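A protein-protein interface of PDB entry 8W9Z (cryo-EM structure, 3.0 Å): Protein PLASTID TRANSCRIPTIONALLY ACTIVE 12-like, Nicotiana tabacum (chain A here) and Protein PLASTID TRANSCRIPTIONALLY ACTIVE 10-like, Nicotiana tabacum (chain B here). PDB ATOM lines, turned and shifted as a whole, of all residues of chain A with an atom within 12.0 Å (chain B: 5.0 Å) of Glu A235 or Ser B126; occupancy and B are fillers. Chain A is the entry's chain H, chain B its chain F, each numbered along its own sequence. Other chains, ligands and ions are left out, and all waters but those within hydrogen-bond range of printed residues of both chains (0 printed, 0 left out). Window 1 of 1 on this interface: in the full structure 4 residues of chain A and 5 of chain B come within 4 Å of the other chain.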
ATOM      1  N   LYS A 229     -14.326 -32.403   1.425  1.00  0.00           N
ATOM      2  CA  LYS A 229     -12.936 -31.966   1.285  1.00  0.00           C
ATOM      3  C   LYS A 229     -12.705 -30.498   1.553  1.00  0.00           C
ATOM      4  O   LYS A 229     -13.387 -29.647   0.992  1.00  0.00           O
ATOM      5  CB  LYS A 229     -12.412 -32.303  -0.108  1.00  0.00           C
ATOM      6  N   PRO A 230     -11.744 -30.192   2.419  1.00  0.00           N
ATOM      7  CA  PRO A 230     -11.395 -28.799   2.692  1.00  0.00           C
ATOM      8  C   PRO A 230     -10.416 -28.253   1.648  1.00  0.00           C
ATOM      9  O   PRO A 230      -9.997 -29.007   0.776  1.00  0.00           O
ATOM     10  CB  PRO A 230     -10.736 -28.873   4.064  1.00  0.00           C
ATOM     11  CG  PRO A 230     -10.936 -30.273   4.558  1.00  0.00           C
ATOM     12  CD  PRO A 230     -11.064 -31.112   3.336  1.00  0.00           C
ATOM     13  N   LEU A 231     -10.064 -26.970   1.720  1.00  0.00           N
ATOM     14  CA  LEU A 231      -9.155 -26.378   0.751  1.00  0.00           C
ATOM     15  C   LEU A 231      -7.844 -27.095   0.798  1.00  0.00           C
ATOM     16  O   LEU A 231      -7.357 -27.434   1.869  1.00  0.00           O
ATOM     17  CB  LEU A 231      -8.901 -24.910   1.052  1.00  0.00           C
ATOM     18  CG  LEU A 231      -9.918 -23.873   0.592  1.00  0.00           C
ATOM     19  CD1 LEU A 231      -9.372 -22.480   0.855  1.00  0.00           C
ATOM     20  CD2 LEU A 231     -10.215 -24.063  -0.883  1.00  0.00           C
ATOM     21  N   THR A 232      -7.258 -27.325  -0.362  1.00  0.00           N
ATOM     22  CA  THR A 232      -5.998 -28.042  -0.443  1.00  0.00           C
ATOM     23  C   THR A 232      -4.860 -27.181   0.026  1.00  0.00           C
ATOM     24  O   THR A 232      -4.978 -25.968   0.067  1.00  0.00           O
ATOM     25  CB  THR A 232      -5.701 -28.453  -1.878  1.00  0.00           C
ATOM     26  OG1 THR A 232      -5.558 -27.276  -2.682  1.00  0.00           O
ATOM     27  CG2 THR A 232      -6.830 -29.300  -2.425  1.00  0.00           C
ATOM     28  N   SER A 233      -3.734 -27.793   0.346  1.00  0.00           N
ATOM     29  CA  SER A 233      -2.622 -27.040   0.890  1.00  0.00           C
ATOM     30  C   SER A 233      -2.183 -25.990  -0.086  1.00  0.00           C
ATOM     31  O   SER A 233      -1.814 -24.894   0.305  1.00  0.00           O
ATOM     32  CB  SER A 233      -1.456 -27.958   1.187  1.00  0.00           C
ATOM     33  OG  SER A 233      -0.909 -28.471  -0.013  1.00  0.00           O
ATOM     34  N   GLU A 234      -2.227 -26.315  -1.360  1.00  0.00           N
ATOM     35  CA  GLU A 234      -1.839 -25.359  -2.357  1.00  0.00           C
ATOM     36  C   GLU A 234      -2.712 -24.134  -2.288  1.00  0.00           C
ATOM     37  O   GLU A 234      -2.227 -23.020  -2.427  1.00  0.00           O
ATOM     38  CB  GLU A 234      -1.976 -25.974  -3.731  1.00  0.00           C
ATOM     39  CG  GLU A 234      -0.671 -26.506  -4.294  1.00  0.00           C
ATOM     40  CD  GLU A 234       0.294 -25.400  -4.688  1.00  0.00           C
ATOM     41  OE1 GLU A 234      -0.151 -24.250  -4.890  1.00  0.00           O
ATOM     42  OE2 GLU A 234       1.505 -25.685  -4.811  1.00  0.00           O
ATOM     43  N   GLU A 235      -3.997 -24.334  -2.049  1.00  0.00           N
ATOM     44  CA  GLU A 235      -4.926 -23.221  -2.069  1.00  0.00           C
ATOM     45  C   GLU A 235      -4.871 -22.289  -0.890  1.00  0.00           C
ATOM     46  O   GLU A 235      -5.419 -21.202  -0.937  1.00  0.00           O
ATOM     47  CB  GLU A 235      -6.331 -23.765  -2.220  1.00  0.00           C
ATOM     48  CG  GLU A 235      -6.937 -23.526  -3.585  1.00  0.00           C
ATOM     49  CD  GLU A 235      -7.308 -22.076  -3.802  1.00  0.00           C
ATOM     50  OE1 GLU A 235      -7.847 -21.452  -2.865  1.00  0.00           O
ATOM     51  OE2 GLU A 235      -7.068 -21.560  -4.910  1.00  0.00           O
ATOM     52  N   LEU A 236      -4.227 -22.701   0.176  1.00  0.00           N
ATOM     53  CA  LEU A 236      -4.191 -21.880   1.358  1.00  0.00           C
ATOM     54  C   LEU A 236      -3.217 -20.744   1.195  1.00  0.00           C
ATOM     55  O   LEU A 236      -2.379 -20.771   0.314  1.00  0.00           O
ATOM     56  CB  LEU A 236      -3.813 -22.710   2.565  1.00  0.00           C
ATOM     57  CG  LEU A 236      -4.585 -23.986   2.856  1.00  0.00           C
ATOM     58  CD1 LEU A 236      -3.866 -24.779   3.930  1.00  0.00           C
ATOM     59  CD2 LEU A 236      -5.996 -23.650   3.292  1.00  0.00           C
ATOM     60  N   TRP A 237      -3.311 -19.739   2.046  1.00  0.00           N
ATOM     61  CA  TRP A 237      -2.379 -18.644   2.004  1.00  0.00           C
ATOM     62  C   TRP A 237      -1.069 -19.177   2.490  1.00  0.00           C
ATOM     63  O   TRP A 237      -1.027 -20.212   3.126  1.00  0.00           O
ATOM     64  CB  TRP A 237      -2.827 -17.537   2.917  1.00  0.00           C
ATOM     65  CG  TRP A 237      -4.032 -16.818   2.487  1.00  0.00           C
ATOM     66  CD1 TRP A 237      -4.429 -16.568   1.213  1.00  0.00           C
ATOM     67  CD2 TRP A 237      -5.000 -16.214   3.339  1.00  0.00           C
ATOM     68  NE1 TRP A 237      -5.599 -15.856   1.218  1.00  0.00           N
ATOM     69  CE2 TRP A 237      -5.969 -15.625   2.515  1.00  0.00           C
ATOM     70  CE3 TRP A 237      -5.146 -16.121   4.723  1.00  0.00           C
ATOM     71  CZ2 TRP A 237      -7.065 -14.953   3.026  1.00  0.00           C
ATOM     72  CZ3 TRP A 237      -6.232 -15.454   5.227  1.00  0.00           C
ATOM     73  CH2 TRP A 237      -7.178 -14.879   4.383  1.00  0.00           C
ATOM     74  N   TRP A 238       0.017 -18.471   2.248  1.00  0.00           N
ATOM     75  CA  TRP A 238       1.328 -18.995   2.582  1.00  0.00           C
ATOM     76  C   TRP A 238       1.521 -19.333   4.035  1.00  0.00           C
ATOM     77  O   TRP A 238       2.175 -20.310   4.350  1.00  0.00           O
ATOM     78  CB  TRP A 238       2.413 -18.035   2.095  1.00  0.00           C
ATOM     79  CG  TRP A 238       2.915 -17.004   3.049  1.00  0.00           C
ATOM     80  CD1 TRP A 238       3.745 -17.193   4.119  1.00  0.00           C
ATOM     81  CD2 TRP A 238       2.680 -15.607   2.974  1.00  0.00           C
ATOM     82  NE1 TRP A 238       4.002 -16.001   4.735  1.00  0.00           N
ATOM     83  CE2 TRP A 238       3.363 -15.009   4.045  1.00  0.00           C
ATOM     84  CE3 TRP A 238       1.944 -14.803   2.111  1.00  0.00           C
ATOM     85  CZ2 TRP A 238       3.332 -13.648   4.272  1.00  0.00           C
ATOM     86  CZ3 TRP A 238       1.917 -13.455   2.336  1.00  0.00           C
ATOM     87  CH2 TRP A 238       2.603 -12.888   3.405  1.00  0.00           C
ATOM     88  N   ASN A 239       0.951 -18.554   4.932  1.00  0.00           N
ATOM     89  CA  ASN A 239       1.182 -18.777   6.334  1.00  0.00           C
ATOM     90  C   ASN A 239       0.718 -20.133   6.753  1.00  0.00           C
ATOM     91  O   ASN A 239       1.334 -20.756   7.591  1.00  0.00           O
ATOM     92  CB  ASN A 239       0.576 -17.685   7.203  1.00  0.00           C
ATOM     93  CG  ASN A 239      -0.838 -17.331   6.824  1.00  0.00           C
ATOM     94  OD1 ASN A 239      -1.277 -17.561   5.706  1.00  0.00           O
ATOM     95  ND2 ASN A 239      -1.562 -16.745   7.766  1.00  0.00           N
ATOM     96  N   TRP A 240      -0.383 -20.596   6.204  1.00  0.00           N
ATOM     97  CA  TRP A 240      -0.914 -21.862   6.642  1.00  0.00           C
ATOM     98  C   TRP A 240      -0.465 -23.050   5.840  1.00  0.00           C
ATOM     99  O   TRP A 240      -0.840 -24.163   6.151  1.00  0.00           O
ATOM    100  CB  TRP A 240      -2.425 -21.817   6.655  1.00  0.00           C
ATOM    101  CG  TRP A 240      -2.977 -20.769   7.528  1.00  0.00           C
ATOM    102  CD1 TRP A 240      -3.559 -19.608   7.139  1.00  0.00           C
ATOM    103  CD2 TRP A 240      -3.007 -20.776   8.954  1.00  0.00           C
ATOM    104  NE1 TRP A 240      -3.948 -18.886   8.233  1.00  0.00           N
ATOM    105  CE2 TRP A 240      -3.619 -19.584   9.362  1.00  0.00           C
ATOM    106  CE3 TRP A 240      -2.573 -21.678   9.926  1.00  0.00           C
ATOM    107  CZ2 TRP A 240      -3.810 -19.268  10.697  1.00  0.00           C
ATOM    108  CZ3 TRP A 240      -2.763 -21.362  11.248  1.00  0.00           C
ATOM    109  CH2 TRP A 240      -3.376 -20.168  11.624  1.00  0.00           C
ATOM    110  N   ARG A 241       0.313 -22.843   4.797  1.00  0.00           N
ATOM    111  CA  ARG A 241       0.686 -23.956   3.947  1.00  0.00           C
ATOM    112  C   ARG A 241       1.627 -24.867   4.680  1.00  0.00           C
ATOM    113  O   ARG A 241       2.439 -24.408   5.463  1.00  0.00           O
ATOM    114  CB  ARG A 241       1.305 -23.458   2.660  1.00  0.00           C
ATOM    115  CG  ARG A 241       1.206 -24.431   1.506  1.00  0.00           C
ATOM    116  CD  ARG A 241       1.497 -23.716   0.205  1.00  0.00           C
ATOM    117  NE  ARG A 241       0.754 -22.466   0.115  1.00  0.00           N
ATOM    118  CZ  ARG A 241       0.853 -21.618  -0.898  1.00  0.00           C
ATOM    119  NH1 ARG A 241       1.662 -21.889  -1.910  1.00  0.00           N
ATOM    120  NH2 ARG A 241       0.147 -20.499  -0.904  1.00  0.00           N
ATOM    121  N   LYS A 242       1.523 -26.164   4.439  1.00  0.00           N
ATOM    122  CA  LYS A 242       2.365 -27.136   5.123  1.00  0.00           C
ATOM    123  C   LYS A 242       3.629 -27.392   4.306  1.00  0.00           C
ATOM    124  O   LYS A 242       3.544 -27.472   3.091  1.00  0.00           O
ATOM    125  CB  LYS A 242       1.598 -28.431   5.306  1.00  0.00           C
ATOM    126  CG  LYS A 242       2.316 -29.505   6.097  1.00  0.00           C
ATOM    127  CD  LYS A 242       1.570 -30.823   6.004  1.00  0.00           C
ATOM    128  CE  LYS A 242       1.425 -31.270   4.559  1.00  0.00           C
ATOM    129  NZ  LYS A 242       2.740 -31.519   3.904  1.00  0.00           N
ATOM    130  N   PRO A 243       4.815 -27.528   4.945  1.00  0.00           N
ATOM    131  CA  PRO A 243       6.000 -27.678   4.094  1.00  0.00           C
ATOM    132  C   PRO A 243       5.980 -28.994   3.331  1.00  0.00           C
ATOM    133  O   PRO A 243       5.397 -29.987   3.770  1.00  0.00           O
ATOM    134  CB  PRO A 243       7.162 -27.629   5.091  1.00  0.00           C
ATOM    135  CG  PRO A 243       6.613 -26.925   6.285  1.00  0.00           C
ATOM    136  CD  PRO A 243       5.172 -27.325   6.358  1.00  0.00           C
ATOM    137  N   GLU A 244       6.633 -28.988   2.167  1.00  0.00           N
ATOM    138  CA  GLU A 244       6.702 -30.196   1.353  1.00  0.00           C
ATOM    139  C   GLU A 244       7.569 -31.258   2.017  1.00  0.00           C
ATOM    140  O   GLU A 244       7.252 -32.452   1.962  1.00  0.00           O
ATOM    141  CB  GLU A 244       7.234 -29.861  -0.040  1.00  0.00           C
ATOM    142  CG  GLU A 244       6.411 -28.826  -0.792  1.00  0.00           C
ATOM    143  CD  GLU A 244       5.047 -29.347  -1.208  1.00  0.00           C
ATOM    144  OE1 GLU A 244       4.872 -30.582  -1.273  1.00  0.00           O
ATOM    145  OE2 GLU A 244       4.149 -28.519  -1.470  1.00  0.00           O
ATOM    146  N   LYS B 123      -6.129 -10.942  -4.034  1.00  0.00           N
ATOM    147  CA  LYS B 123      -6.898 -12.036  -4.617  1.00  0.00           C
ATOM    148  C   LYS B 123      -6.016 -12.992  -5.410  1.00  0.00           C
ATOM    149  O   LYS B 123      -6.331 -14.182  -5.509  1.00  0.00           O
ATOM    150  CB  LYS B 123      -8.014 -11.487  -5.504  1.00  0.00           C
ATOM    151  CG  LYS B 123      -9.214 -10.957  -4.739  1.00  0.00           C
ATOM    152  CD  LYS B 123     -10.300 -10.470  -5.684  1.00  0.00           C
ATOM    153  CE  LYS B 123     -11.592 -10.180  -4.939  1.00  0.00           C
ATOM    154  NZ  LYS B 123     -11.400  -9.185  -3.849  1.00  0.00           N
ATOM    155  N   MET B 124      -4.916 -12.499  -5.978  1.00  0.00           N
ATOM    156  CA  MET B 124      -4.031 -13.339  -6.776  1.00  0.00           C
ATOM    157  C   MET B 124      -3.138 -14.247  -5.938  1.00  0.00           C
ATOM    158  O   MET B 124      -2.254 -14.903  -6.498  1.00  0.00           O
ATOM    159  CB  MET B 124      -3.167 -12.472  -7.696  1.00  0.00           C
ATOM    160  CG  MET B 124      -3.901 -11.934  -8.913  1.00  0.00           C
ATOM    161  SD  MET B 124      -2.842 -10.955  -9.992  1.00  0.00           S
ATOM    162  CE  MET B 124      -1.581 -12.157 -10.406  1.00  0.00           C
ATOM    163  N   LEU B 125      -3.340 -14.305  -4.621  1.00  0.00           N
ATOM    164  CA  LEU B 125      -2.576 -15.220  -3.784  1.00  0.00           C
ATOM    165  C   LEU B 125      -3.090 -16.650  -3.848  1.00  0.00           C
ATOM    166  O   LEU B 125      -2.469 -17.540  -3.256  1.00  0.00           O
ATOM    167  CB  LEU B 125      -2.581 -14.743  -2.330  1.00  0.00           C
ATOM    168  CG  LEU B 125      -1.809 -13.462  -2.021  1.00  0.00           C
ATOM    169  CD1 LEU B 125      -1.840 -13.175  -0.533  1.00  0.00           C
ATOM    170  CD2 LEU B 125      -0.378 -13.565  -2.519  1.00  0.00           C
ATOM    171  N   SER B 126      -4.200 -16.893  -4.542  1.00  0.00           N
ATOM    172  CA  SER B 126      -4.762 -18.231  -4.664  1.00  0.00           C
ATOM    173  C   SER B 126      -4.468 -18.793  -6.044  1.00  0.00           C
ATOM    174  O   SER B 126      -4.629 -18.076  -7.042  1.00  0.00           O
ATOM    175  CB  SER B 126      -6.268 -18.204  -4.426  1.00  0.00           C
ATOM    176  OG  SER B 126      -6.570 -17.680  -3.145  1.00  0.00           O
ATOM    177  N   PRO B 127      -4.032 -20.051  -6.144  1.00  0.00           N
ATOM    178  CA  PRO B 127      -3.732 -20.610  -7.473  1.00  0.00           C
ATOM    179  C   PRO B 127      -4.953 -20.726  -8.370  1.00  0.00           C
ATOM    180  O   PRO B 127      -4.853 -20.482  -9.580  1.00  0.00           O
ATOM    181  CB  PRO B 127      -3.134 -21.985  -7.144  1.00  0.00           C
ATOM    182  CG  PRO B 127      -2.673 -21.879  -5.725  1.00  0.00           C
ATOM    183  CD  PRO B 127      -3.653 -20.968  -5.058  1.00  0.00           C
ATOM    184  N   ASN B 128      -6.106 -21.099  -7.810  1.00  0.00           N
ATOM    185  CA  ASN B 128      -7.307 -21.241  -8.627  1.00  0.00           C
ATOM    186  C   ASN B 128      -7.767 -19.896  -9.174  1.00  0.00           C
ATOM    187  O   ASN B 128      -8.258 -19.818 -10.307  1.00  0.00           O
ATOM    188  CB  ASN B 128      -8.419 -21.906  -7.819  1.00  0.00           C
ATOM    189  CG  ASN B 128      -8.249 -23.409  -7.723  1.00  0.00           C
ATOM    190  OD1 ASN B 128      -8.038 -23.955  -6.642  1.00  0.00           O
ATOM    191  ND2 ASN B 128      -8.346 -24.088  -8.859  1.00  0.00           N
ATOM    192  N   TYR B 129      -7.606 -18.825  -8.396  1.00  0.00           N
ATOM    193  CA  TYR B 129      -7.963 -17.502  -8.897  1.00  0.00           C
ATOM    194  C   TYR B 129      -7.108 -17.126 -10.100  1.00  0.00           C
ATOM    195  O   TYR B 129      -7.615 -16.572 -11.083  1.00  0.00           O
ATOM    196  CB  TYR B 129      -7.822 -16.460  -7.789  1.00  0.00           C
ATOM    197  CG  TYR B 129      -8.187 -15.059  -8.221  1.00  0.00           C
ATOM    198  CD1 TYR B 129      -9.513 -14.651  -8.268  1.00  0.00           C
ATOM    199  CD2 TYR B 129      -7.207 -14.144  -8.582  1.00  0.00           C
ATOM    200  CE1 TYR B 129      -9.852 -13.372  -8.662  1.00  0.00           C
ATOM    201  CE2 TYR B 129      -7.537 -12.862  -8.977  1.00  0.00           C
ATOM    202  CZ  TYR B 129      -8.860 -12.482  -9.016  1.00  0.00           C
ATOM    203  OH  TYR B 129      -9.194 -11.207  -9.409  1.00  0.00           O
ATOM    204  N   ARG B 130      -5.812 -17.435 -10.050  1.00  0.00           N
ATOM    205  CA  ARG B 130      -4.939 -17.135 -11.180  1.00  0.00           C
ATOM    206  C   ARG B 130      -5.271 -18.009 -12.383  1.00  0.00           C
ATOM    207  O   ARG B 130      -5.284 -17.525 -13.523  1.00  0.00           O
ATOM    208  CB  ARG B 130      -3.476 -17.311 -10.774  1.00  0.00           C
ATOM    209  CG  ARG B 130      -3.006 -16.328  -9.716  1.00  0.00           C
ATOM    210  CD  ARG B 130      -1.562 -16.588  -9.324  1.00  0.00           C
ATOM    211  NE  ARG B 130      -1.393 -17.897  -8.700  1.00  0.00           N
ATOM    212  CZ  ARG B 130      -0.236 -18.362  -8.243  1.00  0.00           C
ATOM    213  NH1 ARG B 130       0.863 -17.625  -8.338  1.00  0.00           N
ATOM    214  NH2 ARG B 130      -0.175 -19.566  -7.691  1.00  0.00           N
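Among the printed residues, merely in contact across the chains: Glu A235 with Pro B127 (3.5 Å), Glu A235 with Ser B126 (3.5 Å) and Glu A234 with Pro B127 (3.5 Å).
N of Asn B128 lies within hydrogen-bond range of OE2 of Glu A235 (3.1 Å).
Of chain B, only Ser B126, Pro B127 and Asn B128 come within 4 Å of Glu A235.
No residue of chain A comes within 4 Å of Met B124.
No residue of chain A comes within 4 Å of Leu B125.
Of the printed residues of chain B, Glu A234 touches Pro B127.
Trp A238 touches none of the printed residues of chain B.
The nearest residue of chain A that does not touch Ser B126 is Trp A237 (4.8 Å).
Of the 8 printed residues of chain B, 3 touch a printed residue of chain A.
Hydrophobic or aromatic side chains of chain B within 4 Å of the printed part of chain A: Pro B127.
Printed residues of chain A that touch a printed residue of chain B: Glu A234 and Glu A235.
Among the printed residues, 4 pairs touch across the chains.
Among the printed residues, no Asp or Glu carboxylate lies within 4 Å of a Lys or Arg side-chain nitrogen of the other chain.
The backbone NH (N) of Glu A235 sits at hydrogen-bond distance from the side-chain hydroxyl (OG1) of Thr A232 (3.4 Å).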
